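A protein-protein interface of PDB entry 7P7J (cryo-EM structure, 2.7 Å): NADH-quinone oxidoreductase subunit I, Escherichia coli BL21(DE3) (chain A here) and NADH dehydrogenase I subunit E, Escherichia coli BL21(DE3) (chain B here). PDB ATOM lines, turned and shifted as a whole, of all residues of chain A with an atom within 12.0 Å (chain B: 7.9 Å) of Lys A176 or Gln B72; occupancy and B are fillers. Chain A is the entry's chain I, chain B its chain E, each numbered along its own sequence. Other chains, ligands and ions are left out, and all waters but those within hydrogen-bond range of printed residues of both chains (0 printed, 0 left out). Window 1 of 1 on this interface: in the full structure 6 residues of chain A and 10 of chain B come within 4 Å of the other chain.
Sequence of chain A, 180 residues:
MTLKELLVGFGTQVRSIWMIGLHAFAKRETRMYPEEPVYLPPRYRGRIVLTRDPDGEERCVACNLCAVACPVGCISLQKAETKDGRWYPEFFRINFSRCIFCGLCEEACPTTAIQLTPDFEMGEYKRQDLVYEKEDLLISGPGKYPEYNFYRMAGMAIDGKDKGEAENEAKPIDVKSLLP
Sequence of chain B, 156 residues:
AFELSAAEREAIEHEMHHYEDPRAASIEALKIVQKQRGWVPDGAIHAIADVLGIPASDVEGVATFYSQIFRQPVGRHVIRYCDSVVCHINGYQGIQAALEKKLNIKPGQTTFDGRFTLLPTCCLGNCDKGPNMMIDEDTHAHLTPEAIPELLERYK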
ATOM      1  N   LYS A 171     -12.465  -4.260 -10.190  1.00  0.00           N
ATOM      2  CA  LYS A 171     -12.558  -5.683  -9.926  1.00  0.00           C
ATOM      3  C   LYS A 171     -11.158  -6.289  -9.841  1.00  0.00           C
ATOM      4  O   LYS A 171     -10.242  -5.850 -10.540  1.00  0.00           O
ATOM      5  CB  LYS A 171     -13.358  -6.382 -11.020  1.00  0.00           C
ATOM      6  CG  LYS A 171     -14.773  -5.866 -11.181  1.00  0.00           C
ATOM      7  CD  LYS A 171     -15.750  -6.647 -10.320  1.00  0.00           C
ATOM      8  CE  LYS A 171     -16.592  -5.717  -9.460  1.00  0.00           C
ATOM      9  NZ  LYS A 171     -17.819  -6.387  -8.951  1.00  0.00           N
ATOM     10  N   PRO A 172     -10.960  -7.277  -8.969  1.00  0.00           N
ATOM     11  CA  PRO A 172      -9.630  -7.884  -8.836  1.00  0.00           C
ATOM     12  C   PRO A 172      -9.254  -8.676 -10.079  1.00  0.00           C
ATOM     13  O   PRO A 172     -10.018  -9.519 -10.553  1.00  0.00           O
ATOM     14  CB  PRO A 172      -9.770  -8.790  -7.608  1.00  0.00           C
ATOM     15  CG  PRO A 172     -11.226  -9.017  -7.459  1.00  0.00           C
ATOM     16  CD  PRO A 172     -11.901  -7.785  -7.957  1.00  0.00           C
ATOM     17  N   ILE A 173      -8.067  -8.393 -10.602  1.00  0.00           N
ATOM     18  CA  ILE A 173      -7.527  -9.087 -11.762  1.00  0.00           C
ATOM     19  C   ILE A 173      -6.622 -10.199 -11.257  1.00  0.00           C
ATOM     20  O   ILE A 173      -5.628  -9.934 -10.571  1.00  0.00           O
ATOM     21  CB  ILE A 173      -6.758  -8.129 -12.682  1.00  0.00           C
ATOM     22  CG1 ILE A 173      -7.663  -6.986 -13.136  1.00  0.00           C
ATOM     23  CG2 ILE A 173      -6.199  -8.877 -13.876  1.00  0.00           C
ATOM     24  CD1 ILE A 173      -6.930  -5.897 -13.876  1.00  0.00           C
ATOM     25  N   ASP A 174      -6.966 -11.438 -11.584  1.00  0.00           N
ATOM     26  CA  ASP A 174      -6.136 -12.567 -11.202  1.00  0.00           C
ATOM     27  C   ASP A 174      -4.831 -12.540 -11.986  1.00  0.00           C
ATOM     28  O   ASP A 174      -4.787 -12.124 -13.146  1.00  0.00           O
ATOM     29  CB  ASP A 174      -6.880 -13.880 -11.447  1.00  0.00           C
ATOM     30  CG  ASP A 174      -6.339 -15.028 -10.613  1.00  0.00           C
ATOM     31  OD1 ASP A 174      -7.148 -15.689  -9.929  1.00  0.00           O
ATOM     32  OD2 ASP A 174      -5.117 -15.280 -10.642  1.00  0.00           O
ATOM     33  N   VAL A 175      -3.754 -12.989 -11.337  1.00  0.00           N
ATOM     34  CA  VAL A 175      -2.453 -13.015 -11.995  1.00  0.00           C
ATOM     35  C   VAL A 175      -2.388 -14.093 -13.064  1.00  0.00           C
ATOM     36  O   VAL A 175      -1.507 -14.053 -13.929  1.00  0.00           O
ATOM     37  CB  VAL A 175      -1.327 -13.207 -10.964  1.00  0.00           C
ATOM     38  CG1 VAL A 175      -1.256 -12.010 -10.050  1.00  0.00           C
ATOM     39  CG2 VAL A 175      -1.546 -14.476 -10.164  1.00  0.00           C
ATOM     40  N   LYS A 176      -3.305 -15.052 -13.034  1.00  0.00           N
ATOM     41  CA  LYS A 176      -3.364 -16.119 -14.018  1.00  0.00           C
ATOM     42  C   LYS A 176      -4.126 -15.719 -15.273  1.00  0.00           C
ATOM     43  O   LYS A 176      -4.223 -16.527 -16.200  1.00  0.00           O
ATOM     44  CB  LYS A 176      -4.007 -17.357 -13.389  1.00  0.00           C
ATOM     45  CG  LYS A 176      -3.043 -18.195 -12.554  1.00  0.00           C
ATOM     46  CD  LYS A 176      -3.723 -18.982 -11.432  1.00  0.00           C
ATOM     47  CE  LYS A 176      -5.183 -19.301 -11.713  1.00  0.00           C
ATOM     48  NZ  LYS A 176      -5.330 -20.409 -12.697  1.00  0.00           N
ATOM     49  N   SER A 177      -4.653 -14.496 -15.328  1.00  0.00           N
ATOM     50  CA  SER A 177      -5.480 -14.065 -16.447  1.00  0.00           C
ATOM     51  C   SER A 177      -4.659 -13.918 -17.722  1.00  0.00           C
ATOM     52  O   SER A 177      -3.452 -13.663 -17.689  1.00  0.00           O
ATOM     53  CB  SER A 177      -6.168 -12.741 -16.122  1.00  0.00           C
ATOM     54  OG  SER A 177      -5.221 -11.695 -16.001  1.00  0.00           O
ATOM     55  N   LEU A 178      -5.338 -14.076 -18.859  1.00  0.00           N
ATOM     56  CA  LEU A 178      -4.666 -14.121 -20.152  1.00  0.00           C
ATOM     57  C   LEU A 178      -4.200 -12.750 -20.623  1.00  0.00           C
ATOM     58  O   LEU A 178      -3.263 -12.666 -21.424  1.00  0.00           O
ATOM     59  CB  LEU A 178      -5.597 -14.736 -21.194  1.00  0.00           C
ATOM     60  CG  LEU A 178      -6.206 -16.081 -20.806  1.00  0.00           C
ATOM     61  CD1 LEU A 178      -7.264 -16.491 -21.808  1.00  0.00           C
ATOM     62  CD2 LEU A 178      -5.120 -17.135 -20.707  1.00  0.00           C
ATOM     63  N   LEU A 179      -4.841 -11.682 -20.163  1.00  0.00           N
ATOM     64  CA  LEU A 179      -4.469 -10.345 -20.598  1.00  0.00           C
ATOM     65  C   LEU A 179      -3.103  -9.962 -20.032  1.00  0.00           C
ATOM     66  O   LEU A 179      -2.776 -10.332 -18.901  1.00  0.00           O
ATOM     67  CB  LEU A 179      -5.520  -9.329 -20.157  1.00  0.00           C
ATOM     68  CG  LEU A 179      -6.840  -9.369 -20.924  1.00  0.00           C
ATOM     69  CD1 LEU A 179      -7.875  -8.485 -20.252  1.00  0.00           C
ATOM     70  CD2 LEU A 179      -6.619  -8.943 -22.362  1.00  0.00           C
ATOM     71  N   PRO A 180      -2.277  -9.231 -20.798  1.00  0.00           N
ATOM     72  CA  PRO A 180      -0.957  -8.788 -20.336  1.00  0.00           C
ATOM     73  C   PRO A 180      -1.032  -7.803 -19.173  1.00  0.00           C
ATOM     74  O   PRO A 180      -2.035  -7.103 -19.047  1.00  0.00           O
ATOM     75  CB  PRO A 180      -0.360  -8.111 -21.575  1.00  0.00           C
ATOM     76  CG  PRO A 180      -1.120  -8.667 -22.723  1.00  0.00           C
ATOM     77  CD  PRO A 180      -2.505  -8.879 -22.209  1.00  0.00           C
ATOM     78  N   GLN B  34       2.731 -25.989 -22.474  1.00  0.00           N
ATOM     79  CA  GLN B  34       1.693 -25.212 -23.144  1.00  0.00           C
ATOM     80  C   GLN B  34       1.501 -25.654 -24.590  1.00  0.00           C
ATOM     81  O   GLN B  34       0.370 -25.702 -25.082  1.00  0.00           O
ATOM     82  CB  GLN B  34       2.040 -23.725 -23.078  1.00  0.00           C
ATOM     83  CG  GLN B  34       0.991 -22.820 -23.683  1.00  0.00           C
ATOM     84  CD  GLN B  34       1.360 -21.363 -23.573  1.00  0.00           C
ATOM     85  OE1 GLN B  34       0.760 -20.621 -22.802  1.00  0.00           O
ATOM     86  NE2 GLN B  34       2.351 -20.942 -24.348  1.00  0.00           N
ATOM     87  N   GLY B  38      -2.083 -26.963 -24.819  1.00  0.00           N
ATOM     88  CA  GLY B  38      -2.811 -25.723 -25.048  1.00  0.00           C
ATOM     89  C   GLY B  38      -2.490 -24.625 -24.054  1.00  0.00           C
ATOM     90  O   GLY B  38      -2.380 -23.456 -24.429  1.00  0.00           O
ATOM     91  N   TRP B  39      -2.331 -24.989 -22.785  1.00  0.00           N
ATOM     92  CA  TRP B  39      -2.055 -24.037 -21.721  1.00  0.00           C
ATOM     93  C   TRP B  39      -1.290 -24.762 -20.621  1.00  0.00           C
ATOM     94  O   TRP B  39      -0.921 -25.930 -20.760  1.00  0.00           O
ATOM     95  CB  TRP B  39      -3.349 -23.406 -21.194  1.00  0.00           C
ATOM     96  CG  TRP B  39      -4.283 -24.368 -20.520  1.00  0.00           C
ATOM     97  CD1 TRP B  39      -4.897 -25.449 -21.084  1.00  0.00           C
ATOM     98  CD2 TRP B  39      -4.723 -24.326 -19.160  1.00  0.00           C
ATOM     99  NE1 TRP B  39      -5.683 -26.085 -20.158  1.00  0.00           N
ATOM    100  CE2 TRP B  39      -5.594 -25.415 -18.967  1.00  0.00           C
ATOM    101  CE3 TRP B  39      -4.461 -23.475 -18.083  1.00  0.00           C
ATOM    102  CZ2 TRP B  39      -6.205 -25.674 -17.745  1.00  0.00           C
ATOM    103  CZ3 TRP B  39      -5.070 -23.733 -16.871  1.00  0.00           C
ATOM    104  CH2 TRP B  39      -5.930 -24.824 -16.711  1.00  0.00           C
ATOM    105  N   VAL B  40      -1.047 -24.057 -19.522  1.00  0.00           N
ATOM    106  CA  VAL B  40      -0.326 -24.633 -18.391  1.00  0.00           C
ATOM    107  C   VAL B  40      -1.288 -24.791 -17.219  1.00  0.00           C
ATOM    108  O   VAL B  40      -1.642 -23.798 -16.570  1.00  0.00           O
ATOM    109  CB  VAL B  40       0.885 -23.773 -18.004  1.00  0.00           C
ATOM    110  CG1 VAL B  40       1.609 -24.387 -16.825  1.00  0.00           C
ATOM    111  CG2 VAL B  40       1.824 -23.624 -19.186  1.00  0.00           C
ATOM    112  N   PRO B  41      -1.736 -26.010 -16.914  1.00  0.00           N
ATOM    113  CA  PRO B  41      -2.654 -26.200 -15.782  1.00  0.00           C
ATOM    114  C   PRO B  41      -1.981 -26.048 -14.427  1.00  0.00           C
ATOM    115  O   PRO B  41      -0.773 -25.812 -14.344  1.00  0.00           O
ATOM    116  CB  PRO B  41      -3.177 -27.625 -15.994  1.00  0.00           C
ATOM    117  CG  PRO B  41      -2.139 -28.291 -16.812  1.00  0.00           C
ATOM    118  CD  PRO B  41      -1.559 -27.241 -17.699  1.00  0.00           C
ATOM    119  N   ASP B  42      -2.768 -26.180 -13.355  1.00  0.00           N
ATOM    120  CA  ASP B  42      -2.256 -25.912 -12.013  1.00  0.00           C
ATOM    121  C   ASP B  42      -1.275 -26.985 -11.557  1.00  0.00           C
ATOM    122  O   ASP B  42      -0.289 -26.680 -10.877  1.00  0.00           O
ATOM    123  CB  ASP B  42      -3.415 -25.791 -11.027  1.00  0.00           C
ATOM    124  CG  ASP B  42      -4.367 -24.667 -11.385  1.00  0.00           C
ATOM    125  OD1 ASP B  42      -4.249 -24.118 -12.500  1.00  0.00           O
ATOM    126  OD2 ASP B  42      -5.234 -24.331 -10.552  1.00  0.00           O
ATOM    127  N   ILE B  45       2.603 -26.777 -12.847  1.00  0.00           N
ATOM    128  CA  ILE B  45       3.583 -26.001 -12.091  1.00  0.00           C
ATOM    129  C   ILE B  45       4.331 -26.900 -11.116  1.00  0.00           C
ATOM    130  O   ILE B  45       5.565 -26.877 -11.043  1.00  0.00           O
ATOM    131  CB  ILE B  45       2.887 -24.836 -11.367  1.00  0.00           C
ATOM    132  CG1 ILE B  45       2.209 -23.918 -12.382  1.00  0.00           C
ATOM    133  CG2 ILE B  45       3.875 -24.066 -10.513  1.00  0.00           C
ATOM    134  CD1 ILE B  45       3.171 -23.240 -13.322  1.00  0.00           C
ATOM    135  N   GLU B  60       5.569 -20.771 -10.661  1.00  0.00           N
ATOM    136  CA  GLU B  60       4.328 -20.010 -10.751  1.00  0.00           C
ATOM    137  C   GLU B  60       4.598 -18.537 -11.031  1.00  0.00           C
ATOM    138  O   GLU B  60       3.877 -17.911 -11.815  1.00  0.00           O
ATOM    139  CB  GLU B  60       3.520 -20.174  -9.465  1.00  0.00           C
ATOM    140  CG  GLU B  60       2.185 -19.451  -9.473  1.00  0.00           C
ATOM    141  CD  GLU B  60       1.160 -20.125 -10.359  1.00  0.00           C
ATOM    142  OE1 GLU B  60       1.277 -21.347 -10.581  1.00  0.00           O
ATOM    143  OE2 GLU B  60       0.234 -19.436 -10.833  1.00  0.00           O
ATOM    144  N   ALA B  63       5.529 -18.326 -14.686  1.00  0.00           N
ATOM    145  CA  ALA B  63       4.381 -18.543 -15.561  1.00  0.00           C
ATOM    146  C   ALA B  63       3.423 -17.358 -15.543  1.00  0.00           C
ATOM    147  O   ALA B  63       2.851 -17.000 -16.580  1.00  0.00           O
ATOM    148  CB  ALA B  63       3.652 -19.823 -15.164  1.00  0.00           C
ATOM    149  N   THR B  64       3.230 -16.736 -14.381  1.00  0.00           N
ATOM    150  CA  THR B  64       2.366 -15.570 -14.292  1.00  0.00           C
ATOM    151  C   THR B  64       3.053 -14.289 -14.741  1.00  0.00           C
ATOM    152  O   THR B  64       2.364 -13.311 -15.046  1.00  0.00           O
ATOM    153  CB  THR B  64       1.865 -15.395 -12.861  1.00  0.00           C
ATOM    154  OG1 THR B  64       2.980 -15.442 -11.967  1.00  0.00           O
ATOM    155  CG2 THR B  64       0.888 -16.496 -12.500  1.00  0.00           C
ATOM    156  N   ILE B  69       2.668 -17.348 -21.605  1.00  0.00           N
ATOM    157  CA  ILE B  69       2.494 -18.582 -20.850  1.00  0.00           C
ATOM    158  C   ILE B  69       1.106 -18.526 -20.229  1.00  0.00           C
ATOM    159  O   ILE B  69       0.884 -17.814 -19.244  1.00  0.00           O
ATOM    160  CB  ILE B  69       3.588 -18.757 -19.791  1.00  0.00           C
ATOM    161  CG1 ILE B  69       4.962 -18.782 -20.460  1.00  0.00           C
ATOM    162  CG2 ILE B  69       3.364 -20.032 -19.006  1.00  0.00           C
ATOM    163  CD1 ILE B  69       6.113 -18.750 -19.490  1.00  0.00           C
ATOM    164  N   PHE B  70       0.168 -19.266 -20.808  1.00  0.00           N
ATOM    165  CA  PHE B  70      -1.235 -19.177 -20.430  1.00  0.00           C
ATOM    166  C   PHE B  70      -1.492 -20.042 -19.204  1.00  0.00           C
ATOM    167  O   PHE B  70      -1.188 -21.239 -19.207  1.00  0.00           O
ATOM    168  CB  PHE B  70      -2.132 -19.609 -21.587  1.00  0.00           C
ATOM    169  CG  PHE B  70      -1.933 -18.804 -22.837  1.00  0.00           C
ATOM    170  CD1 PHE B  70      -1.730 -17.437 -22.768  1.00  0.00           C
ATOM    171  CD2 PHE B  70      -1.939 -19.415 -24.077  1.00  0.00           C
ATOM    172  CE1 PHE B  70      -1.542 -16.694 -23.914  1.00  0.00           C
ATOM    173  CE2 PHE B  70      -1.750 -18.678 -25.225  1.00  0.00           C
ATOM    174  CZ  PHE B  70      -1.552 -17.316 -25.144  1.00  0.00           C
ATOM    175  N   ARG B  71      -2.051 -19.435 -18.160  1.00  0.00           N
ATOM    176  CA  ARG B  71      -2.403 -20.143 -16.940  1.00  0.00           C
ATOM    177  C   ARG B  71      -3.908 -20.297 -16.779  1.00  0.00           C
ATOM    178  O   ARG B  71      -4.374 -20.682 -15.703  1.00  0.00           O
ATOM    179  CB  ARG B  71      -1.806 -19.431 -15.728  1.00  0.00           C
ATOM    180  CG  ARG B  71      -0.306 -19.609 -15.586  1.00  0.00           C
ATOM    181  CD  ARG B  71       0.047 -21.019 -15.157  1.00  0.00           C
ATOM    182  NE  ARG B  71      -0.258 -21.257 -13.753  1.00  0.00           N
ATOM    183  CZ  ARG B  71      -1.306 -21.943 -13.320  1.00  0.00           C
ATOM    184  NH1 ARG B  71      -2.171 -22.485 -14.158  1.00  0.00           N
ATOM    185  NH2 ARG B  71      -1.491 -22.086 -12.011  1.00  0.00           N
ATOM    186  N   GLN B  72      -4.675 -20.000 -17.820  1.00  0.00           N
ATOM    187  CA  GLN B  72      -6.111 -20.206 -17.877  1.00  0.00           C
ATOM    188  C   GLN B  72      -6.449 -20.946 -19.161  1.00  0.00           C
ATOM    189  O   GLN B  72      -5.722 -20.828 -20.152  1.00  0.00           O
ATOM    190  CB  GLN B  72      -6.865 -18.869 -17.825  1.00  0.00           C
ATOM    191  CG  GLN B  72      -6.957 -18.274 -16.434  1.00  0.00           C
ATOM    192  CD  GLN B  72      -7.986 -17.169 -16.340  1.00  0.00           C
ATOM    193  OE1 GLN B  72      -8.455 -16.656 -17.355  1.00  0.00           O
ATOM    194  NE2 GLN B  72      -8.339 -16.793 -15.118  1.00  0.00           N
ATOM    195  N   PRO B  73      -7.523 -21.741 -19.165  1.00  0.00           N
ATOM    196  CA  PRO B  73      -7.864 -22.510 -20.371  1.00  0.00           C
ATOM    197  C   PRO B  73      -8.282 -21.599 -21.517  1.00  0.00           C
ATOM    198  O   PRO B  73      -9.103 -20.696 -21.346  1.00  0.00           O
ATOM    199  CB  PRO B  73      -9.021 -23.404 -19.911  1.00  0.00           C
ATOM    200  CG  PRO B  73      -9.552 -22.748 -18.683  1.00  0.00           C
ATOM    201  CD  PRO B  73      -8.371 -22.121 -18.023  1.00  0.00           C
ATOM    202  N   VAL B  74      -7.701 -21.845 -22.689  1.00  0.00           N
ATOM    203  CA  VAL B  74      -7.969 -21.048 -23.880  1.00  0.00           C
ATOM    204  C   VAL B  74      -8.655 -21.920 -24.920  1.00  0.00           C
ATOM    205  O   VAL B  74      -8.845 -23.124 -24.712  1.00  0.00           O
ATOM    206  CB  VAL B  74      -6.675 -20.439 -24.448  1.00  0.00           C
ATOM    207  CG1 VAL B  74      -5.959 -19.629 -23.387  1.00  0.00           C
ATOM    208  CG2 VAL B  74      -5.768 -21.534 -24.977  1.00  0.00           C
ATOM    209  N   GLY B  75      -9.032 -21.320 -26.045  1.00  0.00           N
ATOM    210  CA  GLY B  75      -9.609 -22.064 -27.141  1.00  0.00           C
ATOM    211  C   GLY B  75      -8.556 -22.784 -27.957  1.00  0.00           C
ATOM    212  O   GLY B  75      -7.354 -22.701 -27.703  1.00  0.00           O
ATOM    213  N   GLY B 108      -9.717 -10.911 -24.434  1.00  0.00           N
ATOM    214  CA  GLY B 108      -9.276 -11.547 -23.217  1.00  0.00           C
ATOM    215  C   GLY B 108      -9.985 -12.838 -22.865  1.00  0.00           C
ATOM    216  O   GLY B 108      -9.408 -13.661 -22.145  1.00  0.00           O
ATOM    217  N   GLN B 109     -11.206 -13.052 -23.347  1.00  0.00           N
ATOM    218  CA  GLN B 109     -11.941 -14.267 -23.027  1.00  0.00           C
ATOM    219  C   GLN B 109     -12.141 -15.118 -24.279  1.00  0.00           C
ATOM    220  O   GLN B 109     -11.701 -14.772 -25.379  1.00  0.00           O
ATOM    221  CB  GLN B 109     -13.275 -13.943 -22.348  1.00  0.00           C
ATOM    222  CG  GLN B 109     -14.374 -13.413 -23.252  1.00  0.00           C
ATOM    223  CD  GLN B 109     -14.753 -11.985 -22.932  1.00  0.00           C
ATOM    224  OE1 GLN B 109     -14.123 -11.334 -22.100  1.00  0.00           O
ATOM    225  NE2 GLN B 109     -15.819 -11.507 -23.556  1.00  0.00           N
ATOM    226  N   THR B 110     -12.821 -16.247 -24.093  1.00  0.00           N
ATOM    227  CA  THR B 110     -12.931 -17.297 -25.094  1.00  0.00           C
ATOM    228  C   THR B 110     -14.374 -17.411 -25.570  1.00  0.00           C
ATOM    229  O   THR B 110     -15.309 -17.037 -24.857  1.00  0.00           O
ATOM    230  CB  THR B 110     -12.457 -18.645 -24.514  1.00  0.00           C
ATOM    231  OG1 THR B 110     -11.368 -18.417 -23.612  1.00  0.00           O
ATOM    232  CG2 THR B 110     -11.984 -19.589 -25.612  1.00  0.00           C
ATOM    233  N   THR B 117      -9.833 -17.732 -29.091  1.00  0.00           N
ATOM    234  CA  THR B 117      -9.749 -16.769 -28.002  1.00  0.00           C
ATOM    235  C   THR B 117      -8.968 -15.555 -28.495  1.00  0.00           C
ATOM    236  O   THR B 117      -8.026 -15.687 -29.284  1.00  0.00           O
ATOM    237  CB  THR B 117      -9.138 -17.391 -26.711  1.00  0.00           C
ATOM    238  OG1 THR B 117      -9.615 -16.680 -25.562  1.00  0.00           O
ATOM    239  CG2 THR B 117      -7.617 -17.388 -26.703  1.00  0.00           C
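Among the printed residues, 11 pairs touch across the chains.
Among the printed residues, merely in contact across the chains: Val A175 with Thr B64 (3.7 Å), Lys A176 with Glu B60 (3.9 Å), Lys A176 with Gln B72 (3.3 Å), Ser A177 with Gln B72 (3.99 Å), Leu A178 with Phe B70 (3.98 Å), Leu A178 with Gln B72 (3.8 Å), Leu A178 with Val B74 (3.7 Å), Leu A178 with Gly B108 (3.6 Å) and Leu A179 with Gly B108 (3.8 Å).
Lys A176 touches just these residues of chain B: Asp B42 (3.9 Å), Glu B60 (3.9 Å), Arg B71 (3.2 Å) and Gln B72 (3.3 Å).
Printed residues of chain A within 4 Å of Gln B72: Lys A176 (3.3 Å), Ser A177 (3.99 Å) and Leu A178 (3.8 Å).
No residue of chain A comes within 4 Å of Trp B39.
Of chain A, only Val A175 (3.7 Å) comes within 4 Å of Thr B64.
Phe B70 touches just one residue of chain A: Leu A178 (3.98 Å).
Val B74 touches one residue of chain A.
Of the printed residues of chain B, Leu A178 touches Phe B70, Gln B72, Val B74 and Gly B108.
Of the printed residues of chain A, Asp B42 touches Lys A176.
The nearest printed residue of chain A that does not touch Gln B72 is Asp A174 (4.9 Å).
The nearest printed residue of chain A that does not touch Glu B60 is Val A175 (5.3 Å).
OD1 of Asp B42 lies within salt-bridge range of NZ of Lys A176, at 3.9 Å.
O of Arg B71 sits at hydrogen-bond distance from NZ of Lys A176.
OE1 of Gln B34 sits at hydrogen-bond distance from N of Phe B70 (2.5 Å).
The backbone carbonyl oxygen (O) of Phe B70 is in hydrogen-bond range of the backbone NH (N) of Val B40 (2.8 Å).
The backbone carbonyl oxygen of Val B40 is in hydrogen-bond range of the guanidinium group of Arg B71, at 2.8 Å.
The backbone carbonyl oxygen (O) of Glu B60 lies within hydrogen-bond range of the side-chain hydroxyl (OG1) of Thr B64, at 2.6 Å.
NH2 of Arg B71 lies within salt-bridge range of OE1 of Glu B60 (3.2 Å).
The side-chain hydroxyl (OG) of Ser A177 lies within hydrogen-bond range of the backbone carbonyl oxygen (O) of Asp A174, at 2.9 Å.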
